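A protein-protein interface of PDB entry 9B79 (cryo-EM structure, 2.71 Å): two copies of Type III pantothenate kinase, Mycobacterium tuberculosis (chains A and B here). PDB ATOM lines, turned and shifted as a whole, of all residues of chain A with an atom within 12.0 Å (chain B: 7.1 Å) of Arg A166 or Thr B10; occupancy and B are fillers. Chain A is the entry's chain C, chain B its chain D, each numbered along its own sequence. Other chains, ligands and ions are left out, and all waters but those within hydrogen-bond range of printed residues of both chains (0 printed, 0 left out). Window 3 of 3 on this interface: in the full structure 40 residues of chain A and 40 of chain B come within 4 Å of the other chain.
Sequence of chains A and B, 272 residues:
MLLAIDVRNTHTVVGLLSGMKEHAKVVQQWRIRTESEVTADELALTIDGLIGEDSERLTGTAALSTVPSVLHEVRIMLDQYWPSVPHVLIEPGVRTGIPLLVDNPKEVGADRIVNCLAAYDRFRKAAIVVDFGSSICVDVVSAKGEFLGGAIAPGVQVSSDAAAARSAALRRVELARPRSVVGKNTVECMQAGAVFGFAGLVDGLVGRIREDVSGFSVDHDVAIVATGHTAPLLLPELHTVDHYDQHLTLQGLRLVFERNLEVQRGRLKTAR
The guanidinium group (NH1) of Arg A166 sits at hydrogen-bond distance from the side-chain hydroxyl (OG1) of Thr B10 (2.8 Å). OG of Ser A167 sits at hydrogen-bond distance from ND2 of Asn B9 (3.0 Å).
N of Ala A169 sits close to OG of Ser A167 (3.4 Å). The side-chain hydroxyl of Ser A167 sits at hydrogen-bond distance from the backbone NH of Leu A170, 3.2 Å away. OD1 of Asn B9 lies within hydrogen-bond range of OG1 of Thr B66 (3.1 Å). The side-chain hydroxyl (OG) of Ser B134 sits at hydrogen-bond distance from the side-chain hydroxyl (OG1) of Thr B10 (3.1 Å).
Among the printed residues, pairs that only touch across the chains: Ala A163 with Ser B135 (3.9 Å), Arg A166 with Ser B134 (3.6 Å), Arg A166 with Val B158 (3.6 Å) and Leu A170 with Ser B135 (3.6 Å).
Arg A166 touches just these residues of chain B: Thr B10, Ser B134 and Val B158. Thr B10 touches one residue of chain A. Asn B9 touches one residue of chain A. Of the printed residues of chain B, Ala A163 touches Ser B135. Printed residues of chain B within 4 Å of Leu A170: Ser B135. Of the printed residues of chain A, Ser B135 touches Ala A163 and Leu A170. Of the printed residues of chain B, Ser A167 touches Asn B9. Val B7 touches none of the printed residues of chain A. The nearest residue of chain B that does not touch Arg A166 is Asn B9 (4.2 Å). The nearest printed residue of chain B that does not touch Ala A163 is Val B158 (4.6 Å).
Of the 19 printed residues of chain B, 5 touch a printed residue of chain A. Among the printed residues, no Asp or Glu carboxylate lies within 4 Å of a Lys or Arg side-chain nitrogen of the other chain.
3 positions are printed for both chains. Of the 6 pairs that touch across the chains among the printed residues, none has its exchanged pair printed and touching as well.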
ATOM      1  N   GLN A 157      10.919  -4.961  11.581  1.00  0.00           N
ATOM      2  CA  GLN A 157       9.676  -4.957  10.821  1.00  0.00           C
ATOM      3  C   GLN A 157       9.494  -3.650  10.064  1.00  0.00           C
ATOM      4  O   GLN A 157       9.040  -3.655   8.916  1.00  0.00           O
ATOM      5  CB  GLN A 157       8.491  -5.206  11.753  1.00  0.00           C
ATOM      6  CG  GLN A 157       7.207  -5.579  11.033  1.00  0.00           C
ATOM      7  CD  GLN A 157       7.315  -6.903  10.304  1.00  0.00           C
ATOM      8  OE1 GLN A 157       7.176  -7.966  10.907  1.00  0.00           O
ATOM      9  NE2 GLN A 157       7.560  -6.844   9.000  1.00  0.00           N
ATOM     10  N   VAL A 158       9.838  -2.524  10.692  1.00  0.00           N
ATOM     11  CA  VAL A 158       9.708  -1.230  10.027  1.00  0.00           C
ATOM     12  C   VAL A 158      10.615  -1.164   8.806  1.00  0.00           C
ATOM     13  O   VAL A 158      10.204  -0.708   7.731  1.00  0.00           O
ATOM     14  CB  VAL A 158      10.008  -0.090  11.017  1.00  0.00           C
ATOM     15  CG1 VAL A 158       9.670   1.253  10.397  1.00  0.00           C
ATOM     16  CG2 VAL A 158       9.238  -0.298  12.309  1.00  0.00           C
ATOM     17  N   SER A 159      11.858  -1.631   8.946  1.00  0.00           N
ATOM     18  CA  SER A 159      12.778  -1.634   7.815  1.00  0.00           C
ATOM     19  C   SER A 159      12.304  -2.567   6.709  1.00  0.00           C
ATOM     20  O   SER A 159      12.381  -2.216   5.525  1.00  0.00           O
ATOM     21  CB  SER A 159      14.181  -2.027   8.273  1.00  0.00           C
ATOM     22  OG  SER A 159      14.514  -1.389   9.488  1.00  0.00           O
ATOM     23  N   SER A 160      11.840  -3.769   7.066  1.00  0.00           N
ATOM     24  CA  SER A 160      11.385  -4.697   6.035  1.00  0.00           C
ATOM     25  C   SER A 160      10.161  -4.152   5.305  1.00  0.00           C
ATOM     26  O   SER A 160      10.054  -4.272   4.077  1.00  0.00           O
ATOM     27  CB  SER A 160      11.089  -6.064   6.650  1.00  0.00           C
ATOM     28  OG  SER A 160      11.250  -7.095   5.691  1.00  0.00           O
ATOM     29  N   ASP A 161       9.238  -3.525   6.042  1.00  0.00           N
ATOM     30  CA  ASP A 161       8.076  -2.903   5.417  1.00  0.00           C
ATOM     31  C   ASP A 161       8.483  -1.758   4.500  1.00  0.00           C
ATOM     32  O   ASP A 161       7.911  -1.592   3.417  1.00  0.00           O
ATOM     33  CB  ASP A 161       7.104  -2.410   6.490  1.00  0.00           C
ATOM     34  CG  ASP A 161       6.407  -3.544   7.209  1.00  0.00           C
ATOM     35  OD1 ASP A 161       6.515  -4.698   6.745  1.00  0.00           O
ATOM     36  OD2 ASP A 161       5.748  -3.282   8.238  1.00  0.00           O
ATOM     37  N   ALA A 162       9.452  -0.942   4.924  1.00  0.00           N
ATOM     38  CA  ALA A 162       9.912   0.158   4.083  1.00  0.00           C
ATOM     39  C   ALA A 162      10.556  -0.355   2.803  1.00  0.00           C
ATOM     40  O   ALA A 162      10.327   0.197   1.720  1.00  0.00           O
ATOM     41  CB  ALA A 162      10.892   1.037   4.857  1.00  0.00           C
ATOM     42  N   ALA A 163      11.376  -1.403   2.912  1.00  0.00           N
ATOM     43  CA  ALA A 163      11.974  -2.004   1.725  1.00  0.00           C
ATOM     44  C   ALA A 163      10.904  -2.548   0.789  1.00  0.00           C
ATOM     45  O   ALA A 163      10.995  -2.385  -0.432  1.00  0.00           O
ATOM     46  CB  ALA A 163      12.950  -3.110   2.126  1.00  0.00           C
ATOM     47  N   ALA A 164       9.884  -3.205   1.349  1.00  0.00           N
ATOM     48  CA  ALA A 164       8.791  -3.726   0.533  1.00  0.00           C
ATOM     49  C   ALA A 164       8.029  -2.606  -0.167  1.00  0.00           C
ATOM     50  O   ALA A 164       7.666  -2.732  -1.342  1.00  0.00           O
ATOM     51  CB  ALA A 164       7.847  -4.553   1.402  1.00  0.00           C
ATOM     52  N   ALA A 165       7.773  -1.504   0.542  1.00  0.00           N
ATOM     53  CA  ALA A 165       6.961  -0.430  -0.023  1.00  0.00           C
ATOM     54  C   ALA A 165       7.721   0.345  -1.091  1.00  0.00           C
ATOM     55  O   ALA A 165       7.165   0.654  -2.151  1.00  0.00           O
ATOM     56  CB  ALA A 165       6.491   0.510   1.087  1.00  0.00           C
ATOM     57  N   ARG A 166       8.988   0.677  -0.828  1.00  0.00           N
ATOM     58  CA  ARG A 166       9.728   1.544  -1.741  1.00  0.00           C
ATOM     59  C   ARG A 166      10.023   0.856  -3.067  1.00  0.00           C
ATOM     60  O   ARG A 166      10.047   1.514  -4.112  1.00  0.00           O
ATOM     61  CB  ARG A 166      11.030   2.012  -1.096  1.00  0.00           C
ATOM     62  CG  ARG A 166      11.285   3.501  -1.243  1.00  0.00           C
ATOM     63  CD  ARG A 166      12.719   3.841  -0.892  1.00  0.00           C
ATOM     64  NE  ARG A 166      12.946   5.278  -0.820  1.00  0.00           N
ATOM     65  CZ  ARG A 166      13.362   6.018  -1.838  1.00  0.00           C
ATOM     66  NH1 ARG A 166      13.583   5.489  -3.030  1.00  0.00           N
ATOM     67  NH2 ARG A 166      13.557   7.321  -1.658  1.00  0.00           N
ATOM     68  N   SER A 167      10.250  -0.453  -3.048  1.00  0.00           N
ATOM     69  CA  SER A 167      10.587  -1.191  -4.254  1.00  0.00           C
ATOM     70  C   SER A 167       9.330  -1.778  -4.881  1.00  0.00           C
ATOM     71  O   SER A 167       8.517  -2.402  -4.191  1.00  0.00           O
ATOM     72  CB  SER A 167      11.584  -2.304  -3.934  1.00  0.00           C
ATOM     73  OG  SER A 167      11.736  -3.183  -5.035  1.00  0.00           O
ATOM     74  N   ALA A 168       9.174  -1.569  -6.190  1.00  0.00           N
ATOM     75  CA  ALA A 168       8.050  -2.161  -6.907  1.00  0.00           C
ATOM     76  C   ALA A 168       8.156  -3.680  -6.943  1.00  0.00           C
ATOM     77  O   ALA A 168       7.159  -4.382  -6.737  1.00  0.00           O
ATOM     78  CB  ALA A 168       7.972  -1.594  -8.324  1.00  0.00           C
ATOM     79  N   ALA A 169       9.355  -4.207  -7.203  1.00  0.00           N
ATOM     80  CA  ALA A 169       9.525  -5.651  -7.292  1.00  0.00           C
ATOM     81  C   ALA A 169       9.441  -6.332  -5.935  1.00  0.00           C
ATOM     82  O   ALA A 169       9.135  -7.529  -5.875  1.00  0.00           O
ATOM     83  CB  ALA A 169      10.861  -5.986  -7.958  1.00  0.00           C
ATOM     84  N   LEU A 170       9.708  -5.610  -4.850  1.00  0.00           N
ATOM     85  CA  LEU A 170       9.629  -6.182  -3.516  1.00  0.00           C
ATOM     86  C   LEU A 170       8.219  -6.041  -2.962  1.00  0.00           C
ATOM     87  O   LEU A 170       7.595  -4.982  -3.072  1.00  0.00           O
ATOM     88  CB  LEU A 170      10.628  -5.511  -2.570  1.00  0.00           C
ATOM     89  CG  LEU A 170      12.118  -5.732  -2.839  1.00  0.00           C
ATOM     90  CD1 LEU A 170      12.946  -5.126  -1.721  1.00  0.00           C
ATOM     91  CD2 LEU A 170      12.440  -7.208  -3.008  1.00  0.00           C
ATOM     92  N   ARG A 171       7.723  -7.122  -2.376  1.00  0.00           N
ATOM     93  CA  ARG A 171       6.415  -7.184  -1.744  1.00  0.00           C
ATOM     94  C   ARG A 171       6.557  -7.330  -0.234  1.00  0.00           C
ATOM     95  O   ARG A 171       7.630  -7.646   0.284  1.00  0.00           O
ATOM     96  CB  ARG A 171       5.576  -8.302  -2.374  1.00  0.00           C
ATOM     97  CG  ARG A 171       6.107  -9.708  -2.217  1.00  0.00           C
ATOM     98  CD  ARG A 171       5.203 -10.644  -3.002  1.00  0.00           C
ATOM     99  NE  ARG A 171       5.611 -12.041  -2.946  1.00  0.00           N
ATOM    100  CZ  ARG A 171       6.536 -12.562  -3.741  1.00  0.00           C
ATOM    101  NH1 ARG A 171       7.154 -11.830  -4.654  1.00  0.00           N
ATOM    102  NH2 ARG A 171       6.829 -13.853  -3.639  1.00  0.00           N
ATOM    103  N   ARG A 172       5.455  -7.085   0.472  1.00  0.00           N
ATOM    104  CA  ARG A 172       5.424  -7.303   1.912  1.00  0.00           C
ATOM    105  C   ARG A 172       5.448  -8.787   2.245  1.00  0.00           C
ATOM    106  O   ARG A 172       4.722  -9.587   1.647  1.00  0.00           O
ATOM    107  CB  ARG A 172       4.192  -6.642   2.524  1.00  0.00           C
ATOM    108  CG  ARG A 172       4.483  -5.304   3.183  1.00  0.00           C
ATOM    109  CD  ARG A 172       3.216  -4.493   3.386  1.00  0.00           C
ATOM    110  NE  ARG A 172       2.642  -4.047   2.123  1.00  0.00           N
ATOM    111  CZ  ARG A 172       1.418  -3.553   1.989  1.00  0.00           C
ATOM    112  NH1 ARG A 172       0.596  -3.454   3.022  1.00  0.00           N
ATOM    113  NH2 ARG A 172       1.007  -3.153   0.790  1.00  0.00           N
ATOM    114  N   VAL A 173       6.296  -9.144   3.208  1.00  0.00           N
ATOM    115  CA  VAL A 173       6.592 -10.522   3.568  1.00  0.00           C
ATOM    116  C   VAL A 173       6.375 -10.683   5.066  1.00  0.00           C
ATOM    117  O   VAL A 173       6.461  -9.719   5.833  1.00  0.00           O
ATOM    118  CB  VAL A 173       8.046 -10.891   3.171  1.00  0.00           C
ATOM    119  CG1 VAL A 173       8.328 -12.361   3.367  1.00  0.00           C
ATOM    120  CG2 VAL A 173       8.319 -10.511   1.728  1.00  0.00           C
ATOM    121  N   MET A 190      14.166 -12.043   1.248  1.00  0.00           N
ATOM    122  CA  MET A 190      13.815 -10.923   2.115  1.00  0.00           C
ATOM    123  C   MET A 190      13.741 -11.343   3.578  1.00  0.00           C
ATOM    124  O   MET A 190      14.117 -10.572   4.468  1.00  0.00           O
ATOM    125  CB  MET A 190      12.492 -10.302   1.671  1.00  0.00           C
ATOM    126  CG  MET A 190      12.542  -9.647   0.306  1.00  0.00           C
ATOM    127  SD  MET A 190      10.974  -8.897  -0.155  1.00  0.00           S
ATOM    128  CE  MET A 190      10.896  -7.545   1.014  1.00  0.00           C
ATOM    129  N   VAL B   7      18.506   1.833 -14.456  1.00  0.00           N
ATOM    130  CA  VAL B   7      17.414   2.447 -13.715  1.00  0.00           C
ATOM    131  C   VAL B   7      17.178   1.630 -12.455  1.00  0.00           C
ATOM    132  O   VAL B   7      16.816   0.451 -12.528  1.00  0.00           O
ATOM    133  CB  VAL B   7      16.137   2.536 -14.564  1.00  0.00           C
ATOM    134  CG1 VAL B   7      15.063   3.314 -13.822  1.00  0.00           C
ATOM    135  CG2 VAL B   7      16.437   3.177 -15.904  1.00  0.00           C
ATOM    136  N   ARG B   8      17.385   2.254 -11.303  1.00  0.00           N
ATOM    137  CA  ARG B   8      17.050   1.659 -10.023  1.00  0.00           C
ATOM    138  C   ARG B   8      15.771   2.293  -9.488  1.00  0.00           C
ATOM    139  O   ARG B   8      15.192   3.199 -10.091  1.00  0.00           O
ATOM    140  CB  ARG B   8      18.197   1.815  -9.023  1.00  0.00           C
ATOM    141  CG  ARG B   8      19.501   1.163  -9.435  1.00  0.00           C
ATOM    142  CD  ARG B   8      19.321  -0.319  -9.720  1.00  0.00           C
ATOM    143  NE  ARG B   8      20.296  -1.137  -9.007  1.00  0.00           N
ATOM    144  CZ  ARG B   8      21.576  -1.251  -9.335  1.00  0.00           C
ATOM    145  NH1 ARG B   8      22.092  -0.584 -10.352  1.00  0.00           N
ATOM    146  NH2 ARG B   8      22.358  -2.052  -8.620  1.00  0.00           N
ATOM    147  N   ASN B   9      15.329   1.800  -8.335  1.00  0.00           N
ATOM    148  CA  ASN B   9      14.105   2.293  -7.724  1.00  0.00           C
ATOM    149  C   ASN B   9      14.244   3.719  -7.211  1.00  0.00           C
ATOM    150  O   ASN B   9      13.230   4.401  -7.031  1.00  0.00           O
ATOM    151  CB  ASN B   9      13.702   1.359  -6.585  1.00  0.00           C
ATOM    152  CG  ASN B   9      13.232   0.009  -7.084  1.00  0.00           C
ATOM    153  OD1 ASN B   9      12.777  -0.123  -8.220  1.00  0.00           O
ATOM    154  ND2 ASN B   9      13.384  -1.010  -6.254  1.00  0.00           N
ATOM    155  N   THR B  10      15.467   4.187  -6.983  1.00  0.00           N
ATOM    156  CA  THR B  10      15.709   5.506  -6.410  1.00  0.00           C
ATOM    157  C   THR B  10      16.486   6.433  -7.329  1.00  0.00           C
ATOM    158  O   THR B  10      16.125   7.604  -7.461  1.00  0.00           O
ATOM    159  CB  THR B  10      16.459   5.371  -5.076  1.00  0.00           C
ATOM    160  OG1 THR B  10      15.843   4.350  -4.283  1.00  0.00           O
ATOM    161  CG2 THR B  10      16.420   6.683  -4.310  1.00  0.00           C
ATOM    162  N   HIS B  11      17.544   5.943  -7.973  1.00  0.00           N
ATOM    163  CA  HIS B  11      18.354   6.747  -8.874  1.00  0.00           C
ATOM    164  C   HIS B  11      18.638   5.973 -10.153  1.00  0.00           C
ATOM    165  O   HIS B  11      18.620   4.741 -10.179  1.00  0.00           O
ATOM    166  CB  HIS B  11      19.683   7.173  -8.234  1.00  0.00           C
ATOM    167  CG  HIS B  11      19.528   8.085  -7.059  1.00  0.00           C
ATOM    168  ND1 HIS B  11      19.286   7.624  -5.784  1.00  0.00           N
ATOM    169  CD2 HIS B  11      19.584   9.434  -6.966  1.00  0.00           C
ATOM    170  CE1 HIS B  11      19.200   8.649  -4.956  1.00  0.00           C
ATOM    171  NE2 HIS B  11      19.377   9.759  -5.649  1.00  0.00           N
ATOM    172  N   THR B  12      18.902   6.720 -11.217  1.00  0.00           N
ATOM    173  CA  THR B  12      19.309   6.174 -12.500  1.00  0.00           C
ATOM    174  C   THR B  12      20.748   6.591 -12.771  1.00  0.00           C
ATOM    175  O   THR B  12      21.128   7.742 -12.531  1.00  0.00           O
ATOM    176  CB  THR B  12      18.392   6.664 -13.626  1.00  0.00           C
ATOM    177  OG1 THR B  12      17.046   6.262 -13.352  1.00  0.00           O
ATOM    178  CG2 THR B  12      18.814   6.084 -14.968  1.00  0.00           C
ATOM    179  N   ARG B  31      24.505  10.594 -12.439  1.00  0.00           N
ATOM    180  CA  ARG B  31      23.478   9.989 -11.601  1.00  0.00           C
ATOM    181  C   ARG B  31      22.343  10.985 -11.439  1.00  0.00           C
ATOM    182  O   ARG B  31      22.559  12.105 -10.965  1.00  0.00           O
ATOM    183  CB  ARG B  31      24.041   9.586 -10.235  1.00  0.00           C
ATOM    184  CG  ARG B  31      23.363   8.372  -9.626  1.00  0.00           C
ATOM    185  CD  ARG B  31      24.060   7.931  -8.352  1.00  0.00           C
ATOM    186  NE  ARG B  31      23.731   8.795  -7.223  1.00  0.00           N
ATOM    187  CZ  ARG B  31      23.028   8.409  -6.167  1.00  0.00           C
ATOM    188  NH1 ARG B  31      22.577   7.170  -6.054  1.00  0.00           N
ATOM    189  NH2 ARG B  31      22.777   9.285  -5.200  1.00  0.00           N
ATOM    190  N   ILE B  32      21.138  10.578 -11.833  1.00  0.00           N
ATOM    191  CA  ILE B  32      19.960  11.430 -11.766  1.00  0.00           C
ATOM    192  C   ILE B  32      18.903  10.717 -10.938  1.00  0.00           C
ATOM    193  O   ILE B  32      18.999   9.521 -10.663  1.00  0.00           O
ATOM    194  CB  ILE B  32      19.411  11.779 -13.164  1.00  0.00           C
ATOM    195  CG1 ILE B  32      19.236  10.508 -13.998  1.00  0.00           C
ATOM    196  CG2 ILE B  32      20.332  12.763 -13.868  1.00  0.00           C
ATOM    197  CD1 ILE B  32      18.652  10.748 -15.370  1.00  0.00           C
ATOM    198  N   ARG B  33      17.896  11.472 -10.515  1.00  0.00           N
ATOM    199  CA  ARG B  33      16.737  10.844  -9.901  1.00  0.00           C
ATOM    200  C   ARG B  33      15.879  10.182 -10.972  1.00  0.00           C
ATOM    201  O   ARG B  33      15.832  10.622 -12.124  1.00  0.00           O
ATOM    202  CB  ARG B  33      15.920  11.867  -9.116  1.00  0.00           C
ATOM    203  CG  ARG B  33      16.689  12.511  -7.974  1.00  0.00           C
ATOM    204  CD  ARG B  33      15.860  13.565  -7.257  1.00  0.00           C
ATOM    205  NE  ARG B  33      15.437  14.637  -8.150  1.00  0.00           N
ATOM    206  CZ  ARG B  33      14.774  15.717  -7.760  1.00  0.00           C
ATOM    207  NH1 ARG B  33      14.457  15.912  -6.490  1.00  0.00           N
ATOM    208  NH2 ARG B  33      14.426  16.628  -8.665  1.00  0.00           N
ATOM    209  N   THR B  34      15.201   9.107 -10.586  1.00  0.00           N
ATOM    210  CA  THR B  34      14.275   8.416 -11.470  1.00  0.00           C
ATOM    211  C   THR B  34      12.841   8.776 -11.109  1.00  0.00           C
ATOM    212  O   THR B  34      12.499   8.922  -9.931  1.00  0.00           O
ATOM    213  CB  THR B  34      14.466   6.897 -11.412  1.00  0.00           C
ATOM    214  OG1 THR B  34      13.462   6.257 -12.210  1.00  0.00           O
ATOM    215  CG2 THR B  34      14.358   6.389  -9.996  1.00  0.00           C
ATOM    216  N   GLU B  35      12.014   8.953 -12.133  1.00  0.00           N
ATOM    217  CA  GLU B  35      10.575   9.091 -11.967  1.00  0.00           C
ATOM    218  C   GLU B  35       9.909   7.913 -12.656  1.00  0.00           C
ATOM    219  O   GLU B  35      10.254   7.583 -13.793  1.00  0.00           O
ATOM    220  CB  GLU B  35      10.068  10.412 -12.550  1.00  0.00           C
ATOM    221  CG  GLU B  35      10.714  11.647 -11.951  1.00  0.00           C
ATOM    222  CD  GLU B  35      11.923  12.102 -12.738  1.00  0.00           C
ATOM    223  OE1 GLU B  35      12.318  11.390 -13.684  1.00  0.00           O
ATOM    224  OE2 GLU B  35      12.478  13.171 -12.413  1.00  0.00           O
ATOM    225  N   THR B  66      14.830  -1.729 -13.051  1.00  0.00           N
ATOM    226  CA  THR B  66      14.103  -2.487 -12.042  1.00  0.00           C
ATOM    227  C   THR B  66      12.658  -2.032 -11.910  1.00  0.00           C
ATOM    228  O   THR B  66      11.842  -2.761 -11.337  1.00  0.00           O
ATOM    229  CB  THR B  66      14.797  -2.380 -10.681  1.00  0.00           C
ATOM    230  OG1 THR B  66      14.875  -1.006 -10.284  1.00  0.00           O
ATOM    231  CG2 THR B  66      16.197  -2.967 -10.743  1.00  0.00           C
ATOM    232  N   VAL B  67      12.328  -0.854 -12.427  1.00  0.00           N
ATOM    233  CA  VAL B  67      10.952  -0.373 -12.482  1.00  0.00           C
ATOM    234  C   VAL B  67      10.371  -0.779 -13.833  1.00  0.00           C
ATOM    235  O   VAL B  67      10.953  -0.426 -14.871  1.00  0.00           O
ATOM    236  CB  VAL B  67      10.880   1.144 -12.286  1.00  0.00           C
ATOM    237  CG1 VAL B  67       9.439   1.586 -12.117  1.00  0.00           C
ATOM    238  CG2 VAL B  67      11.716   1.561 -11.089  1.00  0.00           C
ATOM    239  N   GLY B 133      22.156  -0.350  -2.626  1.00  0.00           N
ATOM    240  CA  GLY B 133      21.198   0.446  -3.369  1.00  0.00           C
ATOM    241  C   GLY B 133      20.055   0.927  -2.503  1.00  0.00           C
ATOM    242  O   GLY B 133      20.266   1.316  -1.350  1.00  0.00           O
ATOM    243  N   SER B 134      18.837   0.918  -3.049  1.00  0.00           N
ATOM    244  CA  SER B 134      17.663   1.164  -2.220  1.00  0.00           C
ATOM    245  C   SER B 134      17.480   0.051  -1.201  1.00  0.00           C
ATOM    246  O   SER B 134      17.028   0.300  -0.078  1.00  0.00           O
ATOM    247  CB  SER B 134      16.419   1.302  -3.095  1.00  0.00           C
ATOM    248  OG  SER B 134      15.385   1.979  -2.404  1.00  0.00           O
ATOM    249  N   SER B 135      17.824  -1.173  -1.577  1.00  0.00           N
ATOM    250  CA  SER B 135      18.023  -2.279  -0.658  1.00  0.00           C
ATOM    251  C   SER B 135      19.491  -2.679  -0.691  1.00  0.00           C
ATOM    252  O   SER B 135      20.212  -2.385  -1.646  1.00  0.00           O
ATOM    253  CB  SER B 135      17.141  -3.475  -1.028  1.00  0.00           C
ATOM    254  OG  SER B 135      15.814  -3.291  -0.571  1.00  0.00           O
ATOM    255  N   GLN B 157      19.745   4.289   3.966  1.00  0.00           N
ATOM    256  CA  GLN B 157      19.008   5.547   3.901  1.00  0.00           C
ATOM    257  C   GLN B 157      17.504   5.311   3.967  1.00  0.00           C
ATOM    258  O   GLN B 157      16.782   6.075   4.615  1.00  0.00           O
ATOM    259  CB  GLN B 157      19.382   6.301   2.624  1.00  0.00           C
ATOM    260  CG  GLN B 157      18.568   7.560   2.365  1.00  0.00           C
ATOM    261  CD  GLN B 157      18.996   8.729   3.228  1.00  0.00           C
ATOM    262  OE1 GLN B 157      19.994   8.656   3.944  1.00  0.00           O
ATOM    263  NE2 GLN B 157      18.242   9.822   3.161  1.00  0.00           N
ATOM    264  N   VAL B 158      17.020   4.255   3.309  1.00  0.00           N
ATOM    265  CA  VAL B 158      15.589   3.955   3.310  1.00  0.00           C
ATOM    266  C   VAL B 158      15.110   3.642   4.723  1.00  0.00           C
ATOM    267  O   VAL B 158      14.089   4.167   5.184  1.00  0.00           O
ATOM    268  CB  VAL B 158      15.289   2.796   2.344  1.00  0.00           C
ATOM    269  CG1 VAL B 158      13.799   2.495   2.319  1.00  0.00           C
ATOM    270  CG2 VAL B 158      15.803   3.125   0.954  1.00  0.00           C
ATOM    271  N   ASP B 161      15.241   6.801   6.938  1.00  0.00           N
ATOM    272  CA  ASP B 161      14.134   7.696   6.626  1.00  0.00           C
ATOM    273  C   ASP B 161      12.811   7.150   7.148  1.00  0.00           C
ATOM    274  O   ASP B 161      11.973   7.916   7.631  1.00  0.00           O
ATOM    275  CB  ASP B 161      14.059   7.935   5.118  1.00  0.00           C
ATOM    276  CG  ASP B 161      14.930   9.092   4.669  1.00  0.00           C
ATOM    277  OD1 ASP B 161      15.495   9.785   5.540  1.00  0.00           O
ATOM    278  OD2 ASP B 161      15.048   9.308   3.444  1.00  0.00           O
